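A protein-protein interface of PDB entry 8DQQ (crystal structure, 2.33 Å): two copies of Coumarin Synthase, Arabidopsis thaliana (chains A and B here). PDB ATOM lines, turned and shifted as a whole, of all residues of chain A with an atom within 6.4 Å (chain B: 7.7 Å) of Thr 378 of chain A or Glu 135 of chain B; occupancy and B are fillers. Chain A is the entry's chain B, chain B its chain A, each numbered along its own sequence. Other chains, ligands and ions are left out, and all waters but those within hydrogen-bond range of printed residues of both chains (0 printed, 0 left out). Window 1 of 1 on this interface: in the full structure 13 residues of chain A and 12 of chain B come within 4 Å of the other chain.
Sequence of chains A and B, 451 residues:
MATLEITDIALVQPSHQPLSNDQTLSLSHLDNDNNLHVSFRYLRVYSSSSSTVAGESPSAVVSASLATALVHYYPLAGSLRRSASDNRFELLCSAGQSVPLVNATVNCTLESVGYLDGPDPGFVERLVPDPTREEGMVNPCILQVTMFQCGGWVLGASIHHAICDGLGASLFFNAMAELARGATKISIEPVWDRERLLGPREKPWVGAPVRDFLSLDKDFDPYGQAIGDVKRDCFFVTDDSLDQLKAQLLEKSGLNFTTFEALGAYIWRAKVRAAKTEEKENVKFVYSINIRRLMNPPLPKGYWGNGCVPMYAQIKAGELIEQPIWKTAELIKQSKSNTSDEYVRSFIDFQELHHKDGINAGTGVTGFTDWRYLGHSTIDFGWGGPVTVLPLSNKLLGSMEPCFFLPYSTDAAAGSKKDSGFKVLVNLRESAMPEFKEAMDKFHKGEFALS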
ATOM      1  N   SER A 170      -6.616 -20.870  21.223  1.00  0.00           N
ATOM      2  CA  SER A 170      -5.506 -20.041  20.758  1.00  0.00           C
ATOM      3  C   SER A 170      -4.288 -20.200  21.662  1.00  0.00           C
ATOM      4  O   SER A 170      -3.163 -20.372  21.179  1.00  0.00           O
ATOM      5  CB  SER A 170      -5.933 -18.574  20.673  1.00  0.00           C
ATOM      6  OG  SER A 170      -6.836 -18.367  19.597  1.00  0.00           O
ATOM      7  N   LEU A 171      -4.495 -20.124  22.980  1.00  0.00           N
ATOM      8  CA  LEU A 171      -3.406 -20.339  23.931  1.00  0.00           C
ATOM      9  C   LEU A 171      -2.714 -21.671  23.684  1.00  0.00           C
ATOM     10  O   LEU A 171      -1.479 -21.755  23.698  1.00  0.00           O
ATOM     11  CB  LEU A 171      -3.938 -20.285  25.361  1.00  0.00           C
ATOM     12  CG  LEU A 171      -4.335 -18.946  25.979  1.00  0.00           C
ATOM     13  CD1 LEU A 171      -4.860 -19.159  27.391  1.00  0.00           C
ATOM     14  CD2 LEU A 171      -3.158 -17.981  25.986  1.00  0.00           C
ATOM     15  N   PHE A 173      -2.643 -23.552  20.855  1.00  0.00           N
ATOM     16  CA  PHE A 173      -1.926 -23.612  19.586  1.00  0.00           C
ATOM     17  C   PHE A 173      -0.756 -22.638  19.548  1.00  0.00           C
ATOM     18  O   PHE A 173       0.232 -22.893  18.850  1.00  0.00           O
ATOM     19  CB  PHE A 173      -2.879 -23.353  18.418  1.00  0.00           C
ATOM     20  CG  PHE A 173      -3.716 -24.546  18.046  1.00  0.00           C
ATOM     21  CD1 PHE A 173      -3.135 -25.658  17.461  1.00  0.00           C
ATOM     22  CD2 PHE A 173      -5.083 -24.557  18.276  1.00  0.00           C
ATOM     23  CE1 PHE A 173      -3.896 -26.759  17.119  1.00  0.00           C
ATOM     24  CE2 PHE A 173      -5.850 -25.660  17.935  1.00  0.00           C
ATOM     25  CZ  PHE A 173      -5.254 -26.759  17.355  1.00  0.00           C
ATOM     26  N   ASN A 174      -0.842 -21.523  20.277  1.00  0.00           N
ATOM     27  CA  ASN A 174       0.331 -20.667  20.426  1.00  0.00           C
ATOM     28  C   ASN A 174       1.412 -21.351  21.249  1.00  0.00           C
ATOM     29  O   ASN A 174       2.599 -21.066  21.063  1.00  0.00           O
ATOM     30  CB  ASN A 174      -0.051 -19.329  21.061  1.00  0.00           C
ATOM     31  CG  ASN A 174      -0.541 -18.320  20.042  1.00  0.00           C
ATOM     32  OD1 ASN A 174       0.239 -17.793  19.248  1.00  0.00           O
ATOM     33  ND2 ASN A 174      -1.838 -18.042  20.059  1.00  0.00           N
ATOM     34  N   ALA A 177       2.981 -23.812  18.786  1.00  0.00           N
ATOM     35  CA  ALA A 177       3.741 -23.080  17.776  1.00  0.00           C
ATOM     36  C   ALA A 177       5.076 -22.591  18.327  1.00  0.00           C
ATOM     37  O   ALA A 177       6.120 -22.755  17.685  1.00  0.00           O
ATOM     38  CB  ALA A 177       2.919 -21.906  17.246  1.00  0.00           C
ATOM     39  N   GLU A 178       5.062 -21.970  19.512  1.00  0.00           N
ATOM     40  CA  GLU A 178       6.303 -21.440  20.070  1.00  0.00           C
ATOM     41  C   GLU A 178       7.280 -22.562  20.397  1.00  0.00           C
ATOM     42  O   GLU A 178       8.491 -22.411  20.202  1.00  0.00           O
ATOM     43  CB  GLU A 178       6.014 -20.584  21.307  1.00  0.00           C
ATOM     44  CG  GLU A 178       5.419 -21.336  22.490  1.00  0.00           C
ATOM     45  CD  GLU A 178       4.971 -20.414  23.602  1.00  0.00           C
ATOM     46  OE1 GLU A 178       5.067 -19.181  23.424  1.00  0.00           O
ATOM     47  OE2 GLU A 178       4.521 -20.922  24.650  1.00  0.00           O
ATOM     48  N   ARG A 181       9.113 -23.437  17.422  1.00  0.00           N
ATOM     49  CA  ARG A 181      10.077 -22.402  17.089  1.00  0.00           C
ATOM     50  C   ARG A 181      11.255 -22.367  18.054  1.00  0.00           C
ATOM     51  O   ARG A 181      12.045 -21.419  18.009  1.00  0.00           O
ATOM     52  CB  ARG A 181       9.390 -21.033  17.047  1.00  0.00           C
ATOM     53  CG  ARG A 181       8.274 -20.943  16.015  1.00  0.00           C
ATOM     54  CD  ARG A 181       7.861 -19.500  15.749  1.00  0.00           C
ATOM     55  NE  ARG A 181       7.442 -18.792  16.955  1.00  0.00           N
ATOM     56  CZ  ARG A 181       6.221 -18.836  17.470  1.00  0.00           C
ATOM     57  NH1 ARG A 181       5.272 -19.590  16.936  1.00  0.00           N
ATOM     58  NH2 ARG A 181       5.944 -18.107  18.548  1.00  0.00           N
ATOM     59  N   SER A 187       4.972 -19.918  27.314  1.00  0.00           N
ATOM     60  CA  SER A 187       5.012 -18.556  27.837  1.00  0.00           C
ATOM     61  C   SER A 187       3.957 -18.327  28.911  1.00  0.00           C
ATOM     62  O   SER A 187       4.172 -17.531  29.832  1.00  0.00           O
ATOM     63  CB  SER A 187       4.834 -17.558  26.692  1.00  0.00           C
ATOM     64  OG  SER A 187       5.704 -17.869  25.614  1.00  0.00           O
ATOM     65  N   GLY A 375      -4.902 -13.275  16.640  1.00  0.00           N
ATOM     66  CA  GLY A 375      -3.516 -13.351  16.232  1.00  0.00           C
ATOM     67  C   GLY A 375      -3.239 -14.620  15.457  1.00  0.00           C
ATOM     68  O   GLY A 375      -2.526 -15.506  15.940  1.00  0.00           O
ATOM     69  N   HIS A 376      -3.819 -14.732  14.259  1.00  0.00           N
ATOM     70  CA  HIS A 376      -3.625 -15.938  13.463  1.00  0.00           C
ATOM     71  C   HIS A 376      -2.182 -16.077  13.010  1.00  0.00           C
ATOM     72  O   HIS A 376      -1.702 -17.199  12.812  1.00  0.00           O
ATOM     73  CB  HIS A 376      -4.553 -15.931  12.247  1.00  0.00           C
ATOM     74  CG  HIS A 376      -6.001 -16.092  12.588  1.00  0.00           C
ATOM     75  ND1 HIS A 376      -6.534 -17.287  13.017  1.00  0.00           N
ATOM     76  CD2 HIS A 376      -7.029 -15.213  12.547  1.00  0.00           C
ATOM     77  CE1 HIS A 376      -7.829 -17.136  13.236  1.00  0.00           C
ATOM     78  NE2 HIS A 376      -8.154 -15.886  12.958  1.00  0.00           N
ATOM     79  N   SER A 377      -1.476 -14.954  12.851  1.00  0.00           N
ATOM     80  CA  SER A 377      -0.126 -14.991  12.301  1.00  0.00           C
ATOM     81  C   SER A 377       0.851 -15.708  13.225  1.00  0.00           C
ATOM     82  O   SER A 377       1.793 -16.346  12.744  1.00  0.00           O
ATOM     83  CB  SER A 377       0.361 -13.570  12.016  1.00  0.00           C
ATOM     84  OG  SER A 377       0.457 -12.811  13.208  1.00  0.00           O
ATOM     85  N   THR A 378       0.639 -15.636  14.539  1.00  0.00           N
ATOM     86  CA  THR A 378       1.583 -16.200  15.498  1.00  0.00           C
ATOM     87  C   THR A 378       1.459 -17.712  15.655  1.00  0.00           C
ATOM     88  O   THR A 378       2.212 -18.296  16.440  1.00  0.00           O
ATOM     89  CB  THR A 378       1.422 -15.530  16.866  1.00  0.00           C
ATOM     90  OG1 THR A 378       0.069 -15.667  17.320  1.00  0.00           O
ATOM     91  CG2 THR A 378       1.770 -14.048  16.776  1.00  0.00           C
ATOM     92  N   ILE A 379       0.543 -18.353  14.936  1.00  0.00           N
ATOM     93  CA  ILE A 379       0.477 -19.823  14.909  1.00  0.00           C
ATOM     94  C   ILE A 379       1.412 -20.255  13.787  1.00  0.00           C
ATOM     95  O   ILE A 379       1.002 -20.660  12.696  1.00  0.00           O
ATOM     96  CB  ILE A 379      -0.954 -20.335  14.728  1.00  0.00           C
ATOM     97  CG1 ILE A 379      -1.887 -19.659  15.732  1.00  0.00           C
ATOM     98  CG2 ILE A 379      -1.005 -21.847  14.900  1.00  0.00           C
ATOM     99  CD1 ILE A 379      -1.522 -19.931  17.171  1.00  0.00           C
ATOM    100  N   ASP A 380       2.710 -20.162  14.065  1.00  0.00           N
ATOM    101  CA  ASP A 380       3.761 -20.407  13.087  1.00  0.00           C
ATOM    102  C   ASP A 380       4.618 -21.563  13.582  1.00  0.00           C
ATOM    103  O   ASP A 380       5.200 -21.486  14.669  1.00  0.00           O
ATOM    104  CB  ASP A 380       4.604 -19.146  12.878  1.00  0.00           C
ATOM    105  CG  ASP A 380       5.594 -19.277  11.735  1.00  0.00           C
ATOM    106  OD1 ASP A 380       5.934 -20.415  11.347  1.00  0.00           O
ATOM    107  OD2 ASP A 380       6.046 -18.229  11.230  1.00  0.00           O
ATOM    108  N   PHE A 381       4.698 -22.625  12.783  1.00  0.00           N
ATOM    109  CA  PHE A 381       5.533 -23.778  13.098  1.00  0.00           C
ATOM    110  C   PHE A 381       6.852 -23.794  12.341  1.00  0.00           C
ATOM    111  O   PHE A 381       7.613 -24.756  12.477  1.00  0.00           O
ATOM    112  CB  PHE A 381       4.774 -25.079  12.809  1.00  0.00           C
ATOM    113  CG  PHE A 381       3.561 -25.286  13.668  1.00  0.00           C
ATOM    114  CD1 PHE A 381       2.340 -24.747  13.300  1.00  0.00           C
ATOM    115  CD2 PHE A 381       3.640 -26.029  14.836  1.00  0.00           C
ATOM    116  CE1 PHE A 381       1.219 -24.938  14.083  1.00  0.00           C
ATOM    117  CE2 PHE A 381       2.519 -26.223  15.624  1.00  0.00           C
ATOM    118  CZ  PHE A 381       1.308 -25.675  15.246  1.00  0.00           C
ATOM    119  N   GLY A 385       3.042 -18.013   9.144  1.00  0.00           N
ATOM    120  CA  GLY A 385       1.677 -18.044   9.602  1.00  0.00           C
ATOM    121  C   GLY A 385       0.776 -18.621   8.530  1.00  0.00           C
ATOM    122  O   GLY A 385       1.181 -18.785   7.374  1.00  0.00           O
ATOM    123  N   PRO A 386      -0.467 -18.943   8.890  1.00  0.00           N
ATOM    124  CA  PRO A 386      -1.388 -19.528   7.909  1.00  0.00           C
ATOM    125  C   PRO A 386      -1.763 -18.513   6.841  1.00  0.00           C
ATOM    126  O   PRO A 386      -2.028 -17.347   7.138  1.00  0.00           O
ATOM    127  CB  PRO A 386      -2.608 -19.923   8.753  1.00  0.00           C
ATOM    128  CG  PRO A 386      -2.168 -19.813  10.190  1.00  0.00           C
ATOM    129  CD  PRO A 386      -1.095 -18.774  10.208  1.00  0.00           C
ATOM    130  N   HIS B  37      14.871 -10.192  25.462  1.00  0.00           N
ATOM    131  CA  HIS B  37      13.904 -11.047  24.775  1.00  0.00           C
ATOM    132  C   HIS B  37      12.506 -10.729  25.317  1.00  0.00           C
ATOM    133  O   HIS B  37      11.857 -11.532  25.991  1.00  0.00           O
ATOM    134  CB  HIS B  37      14.259 -12.518  24.962  1.00  0.00           C
ATOM    135  CG  HIS B  37      13.322 -13.456  24.269  1.00  0.00           C
ATOM    136  ND1 HIS B  37      12.367 -13.019  23.377  1.00  0.00           N
ATOM    137  CD2 HIS B  37      13.179 -14.801  24.344  1.00  0.00           C
ATOM    138  CE1 HIS B  37      11.678 -14.053  22.930  1.00  0.00           C
ATOM    139  NE2 HIS B  37      12.151 -15.147  23.499  1.00  0.00           N
ATOM    140  N   SER B  39       8.994  -7.711  24.359  1.00  0.00           N
ATOM    141  CA  SER B  39       8.413  -6.686  23.500  1.00  0.00           C
ATOM    142  C   SER B  39       8.210  -5.416  24.313  1.00  0.00           C
ATOM    143  O   SER B  39       7.503  -5.432  25.326  1.00  0.00           O
ATOM    144  CB  SER B  39       7.083  -7.151  22.907  1.00  0.00           C
ATOM    145  OG  SER B  39       7.301  -8.022  21.813  1.00  0.00           O
ATOM    146  N   LEU B  80      12.164 -13.020  13.801  1.00  0.00           N
ATOM    147  CA  LEU B  80      13.218 -13.417  14.722  1.00  0.00           C
ATOM    148  C   LEU B  80      13.134 -14.924  14.934  1.00  0.00           C
ATOM    149  O   LEU B  80      12.117 -15.432  15.420  1.00  0.00           O
ATOM    150  CB  LEU B  80      13.084 -12.677  16.050  1.00  0.00           C
ATOM    151  CG  LEU B  80      13.538 -11.222  16.132  1.00  0.00           C
ATOM    152  CD1 LEU B  80      12.970 -10.586  17.382  1.00  0.00           C
ATOM    153  CD2 LEU B  80      15.053 -11.159  16.153  1.00  0.00           C
ATOM    154  N   ASP B 130      -0.175  -6.309  22.409  1.00  0.00           N
ATOM    155  CA  ASP B 130       0.548  -6.821  23.572  1.00  0.00           C
ATOM    156  C   ASP B 130       0.939  -8.272  23.326  1.00  0.00           C
ATOM    157  O   ASP B 130       0.376  -9.196  23.925  1.00  0.00           O
ATOM    158  CB  ASP B 130      -0.306  -6.685  24.831  1.00  0.00           C
ATOM    159  CG  ASP B 130       0.457  -7.006  26.097  1.00  0.00           C
ATOM    160  OD1 ASP B 130       1.222  -6.141  26.574  1.00  0.00           O
ATOM    161  OD2 ASP B 130       0.285  -8.126  26.622  1.00  0.00           O
ATOM    162  N   PRO B 131       1.915  -8.508  22.453  1.00  0.00           N
ATOM    163  CA  PRO B 131       2.338  -9.880  22.170  1.00  0.00           C
ATOM    164  C   PRO B 131       3.244 -10.423  23.253  1.00  0.00           C
ATOM    165  O   PRO B 131       3.966  -9.690  23.935  1.00  0.00           O
ATOM    166  CB  PRO B 131       3.102  -9.755  20.847  1.00  0.00           C
ATOM    167  CG  PRO B 131       3.521  -8.306  20.766  1.00  0.00           C
ATOM    168  CD  PRO B 131       2.825  -7.523  21.850  1.00  0.00           C
ATOM    169  N   THR B 132       3.202 -11.742  23.396  1.00  0.00           N
ATOM    170  CA  THR B 132       4.134 -12.402  24.289  1.00  0.00           C
ATOM    171  C   THR B 132       5.539 -12.308  23.690  1.00  0.00           C
ATOM    172  O   THR B 132       5.738 -11.787  22.586  1.00  0.00           O
ATOM    173  CB  THR B 132       3.695 -13.849  24.532  1.00  0.00           C
ATOM    174  OG1 THR B 132       4.149 -14.276  25.826  1.00  0.00           O
ATOM    175  CG2 THR B 132       4.260 -14.776  23.468  1.00  0.00           C
ATOM    176  N   ARG B 133       6.532 -12.804  24.433  1.00  0.00           N
ATOM    177  CA  ARG B 133       7.905 -12.695  23.963  1.00  0.00           C
ATOM    178  C   ARG B 133       8.169 -13.597  22.759  1.00  0.00           C
ATOM    179  O   ARG B 133       8.945 -13.223  21.868  1.00  0.00           O
ATOM    180  CB  ARG B 133       8.877 -13.004  25.109  1.00  0.00           C
ATOM    181  CG  ARG B 133       8.765 -14.395  25.698  1.00  0.00           C
ATOM    182  CD  ARG B 133      10.065 -14.791  26.382  1.00  0.00           C
ATOM    183  NE  ARG B 133      10.006 -14.688  27.836  1.00  0.00           N
ATOM    184  CZ  ARG B 133       9.386 -15.559  28.618  1.00  0.00           C
ATOM    185  NH1 ARG B 133       8.693 -16.569  28.112  1.00  0.00           N
ATOM    186  NH2 ARG B 133       9.461 -15.416  29.940  1.00  0.00           N
ATOM    187  N   GLU B 134       7.527 -14.765  22.696  1.00  0.00           N
ATOM    188  CA  GLU B 134       7.691 -15.641  21.538  1.00  0.00           C
ATOM    189  C   GLU B 134       6.887 -15.137  20.344  1.00  0.00           C
ATOM    190  O   GLU B 134       7.399 -15.092  19.221  1.00  0.00           O
ATOM    191  CB  GLU B 134       7.291 -17.075  21.895  1.00  0.00           C
ATOM    192  CG  GLU B 134       8.055 -17.664  23.071  1.00  0.00           C
ATOM    193  CD  GLU B 134       9.534 -17.855  22.783  1.00  0.00           C
ATOM    194  OE1 GLU B 134       9.884 -18.191  21.629  1.00  0.00           O
ATOM    195  OE2 GLU B 134      10.346 -17.677  23.715  1.00  0.00           O
ATOM    196  N   GLU B 135       5.620 -14.768  20.574  1.00  0.00           N
ATOM    197  CA  GLU B 135       4.818 -14.110  19.543  1.00  0.00           C
ATOM    198  C   GLU B 135       5.527 -12.870  19.016  1.00  0.00           C
ATOM    199  O   GLU B 135       5.495 -12.588  17.813  1.00  0.00           O
ATOM    200  CB  GLU B 135       3.440 -13.715  20.088  1.00  0.00           C
ATOM    201  CG  GLU B 135       2.503 -14.866  20.432  1.00  0.00           C
ATOM    202  CD  GLU B 135       1.387 -14.431  21.367  1.00  0.00           C
ATOM    203  OE1 GLU B 135       1.367 -13.243  21.751  1.00  0.00           O
ATOM    204  OE2 GLU B 135       0.535 -15.276  21.719  1.00  0.00           O
ATOM    205  N   GLY B 136       6.177 -12.116  19.908  1.00  0.00           N
ATOM    206  CA  GLY B 136       6.910 -10.932  19.495  1.00  0.00           C
ATOM    207  C   GLY B 136       8.048 -11.221  18.541  1.00  0.00           C
ATOM    208  O   GLY B 136       8.532 -10.307  17.869  1.00  0.00           O
ATOM    209  N   MET B 137       8.490 -12.476  18.461  1.00  0.00           N
ATOM    210  CA  MET B 137       9.528 -12.822  17.502  1.00  0.00           C
ATOM    211  C   MET B 137       8.958 -13.030  16.106  1.00  0.00           C
ATOM    212  O   MET B 137       9.668 -12.828  15.114  1.00  0.00           O
ATOM    213  CB  MET B 137      10.270 -14.078  17.959  1.00  0.00           C
ATOM    214  CG  MET B 137      10.821 -14.002  19.371  1.00  0.00           C
ATOM    215  SD  MET B 137      11.505 -15.582  19.895  1.00  0.00           S
ATOM    216  CE  MET B 137      12.748 -15.843  18.636  1.00  0.00           C
ATOM    217  N   VAL B 138       7.690 -13.430  16.006  1.00  0.00           N
ATOM    218  CA  VAL B 138       7.058 -13.549  14.697  1.00  0.00           C
ATOM    219  C   VAL B 138       6.782 -12.167  14.115  1.00  0.00           C
ATOM    220  O   VAL B 138       7.029 -11.915  12.931  1.00  0.00           O
ATOM    221  CB  VAL B 138       5.772 -14.386  14.800  1.00  0.00           C
ATOM    222  CG1 VAL B 138       5.169 -14.595  13.421  1.00  0.00           C
ATOM    223  CG2 VAL B 138       6.060 -15.717  15.471  1.00  0.00           C
ATOM    224  N   ASN B 139       6.269 -11.252  14.938  1.00  0.00           N
ATOM    225  CA  ASN B 139       5.964  -9.880  14.535  1.00  0.00           C
ATOM    226  C   ASN B 139       6.762  -8.940  15.426  1.00  0.00           C
ATOM    227  O   ASN B 139       6.264  -8.487  16.469  1.00  0.00           O
ATOM    228  CB  ASN B 139       4.467  -9.607  14.636  1.00  0.00           C
ATOM    229  CG  ASN B 139       3.648 -10.534  13.756  1.00  0.00           C
ATOM    230  OD1 ASN B 139       3.924 -10.678  12.567  1.00  0.00           O
ATOM    231  ND2 ASN B 139       2.657 -11.190  14.344  1.00  0.00           N
ATOM    232  N   PRO B 140       8.009  -8.631  15.066  1.00  0.00           N
ATOM    233  CA  PRO B 140       8.838  -7.826  15.976  1.00  0.00           C
ATOM    234  C   PRO B 140       8.412  -6.374  16.049  1.00  0.00           C
ATOM    235  O   PRO B 140       8.380  -5.802  17.145  1.00  0.00           O
ATOM    236  CB  PRO B 140      10.250  -7.975  15.391  1.00  0.00           C
ATOM    237  CG  PRO B 140      10.172  -9.104  14.405  1.00  0.00           C
ATOM    238  CD  PRO B 140       8.768  -9.107  13.899  1.00  0.00           C
ATOM    239  N   ILE B 142       5.507  -3.658  15.435  1.00  0.00           N
ATOM    240  CA  ILE B 142       4.072  -3.478  15.225  1.00  0.00           C
ATOM    241  C   ILE B 142       3.736  -2.026  15.534  1.00  0.00           C
ATOM    242  O   ILE B 142       3.872  -1.586  16.681  1.00  0.00           O
ATOM    243  CB  ILE B 142       3.226  -4.426  16.090  1.00  0.00           C
ATOM    244  CG1 ILE B 142       3.648  -5.878  15.863  1.00  0.00           C
ATOM    245  CG2 ILE B 142       1.753  -4.261  15.764  1.00  0.00           C
ATOM    246  CD1 ILE B 142       2.853  -6.887  16.672  1.00  0.00           C
ATOM    247  N   HIS B 160      10.268  -5.643  19.518  1.00  0.00           N
ATOM    248  CA  HIS B 160      11.099  -6.592  20.241  1.00  0.00           C
ATOM    249  C   HIS B 160      12.461  -5.971  20.514  1.00  0.00           C
ATOM    250  O   HIS B 160      13.111  -5.450  19.603  1.00  0.00           O
ATOM    251  CB  HIS B 160      11.241  -7.886  19.444  1.00  0.00           C
ATOM    252  CG  HIS B 160      11.767  -9.035  20.243  1.00  0.00           C
ATOM    253  ND1 HIS B 160      13.108  -9.200  20.514  1.00  0.00           N
ATOM    254  CD2 HIS B 160      11.135 -10.082  20.822  1.00  0.00           C
ATOM    255  CE1 HIS B 160      13.278 -10.296  21.230  1.00  0.00           C
ATOM    256  NE2 HIS B 160      12.096 -10.851  21.431  1.00  0.00           N
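The side-chain carboxylate (OE2) of Glu 134 of chain B lies within hydrogen-bond range of a ring nitrogen (NE2) of His 37 of chain B (3.1 Å).
NH1 of Arg 181 of chain A sits at hydrogen-bond distance from O of Asp 380 of chain A, at 3.0 Å.
The side-chain hydroxyl of Thr 378 of chain A lies within hydrogen-bond range of the backbone carbonyl oxygen of Gly 375 of chain A.
The backbone NH of Thr 132 of chain B lies within hydrogen-bond range of the side-chain carboxylate of Glu 135 of chain B (2.9 Å).
OE1 of Glu 178 of chain A sits at hydrogen-bond distance from OG of Ser 187 of chain A (2.6 Å).
NH1 of Arg 181 of chain A sits at hydrogen-bond distance from O of Thr 378 of chain A, 3.4 Å away.
Among the printed residues, pairs that only touch across the chains: Asn 174 of chain A with Glu 135 of chain B, Glu 178 of chain A with Glu 134 of chain B, Arg 181 of chain A with Glu 135 of chain B, Arg 181 of chain A with Val 138 of chain B, Ser 187 of chain A with Thr 132 of chain B, Ser 187 of chain A with Glu 134 of chain B, Ser 377 of chain A with Val 138 of chain B, Thr 378 of chain A with Glu 135 of chain B and Thr 378 of chain A with Asn 139 of chain B.
Along chain A the printed residues that touch a printed residue of chain B span positions 174 to 378.
Hydrophobic or aromatic side chains of chain B that line the printed part of chain A: Val 138.
Among the printed residues, 11 pairs touch across the chains.
No position is printed for both chains.
The guanidinium group (NH2) of Arg 181 of chain A sits at hydrogen-bond distance from the backbone carbonyl oxygen (O) of Glu 134 of chain B.
The side-chain amide nitrogen (ND2) of Asn 139 of chain B sits at hydrogen-bond distance from the side-chain hydroxyl (OG) of Ser 377 of chain A, 3.0 Å away.
Thr 378 of chain A touches two residues of chain B.
Printed residues of chain A within 4 Å of Glu 135 of chain B: Asn 174, Arg 181 and Thr 378.
Of the printed residues of chain A, Val 138 of chain B touches Arg 181 (3.7 Å) and Ser 377 (3.9 Å).
Of the printed residues of chain B, Ser 187 of chain A touches Thr 132 and Glu 134.
Printed residues of chain A within 4 Å of Asn 139 of chain B: Ser 377 and Thr 378.
Printed residues of chain B within 4 Å of Asn 174 of chain A: Glu 135 (3.5 Å).
The nearest residue of chain A that does not touch Glu 135 of chain B is Glu 178 of chain A (5.3 Å).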
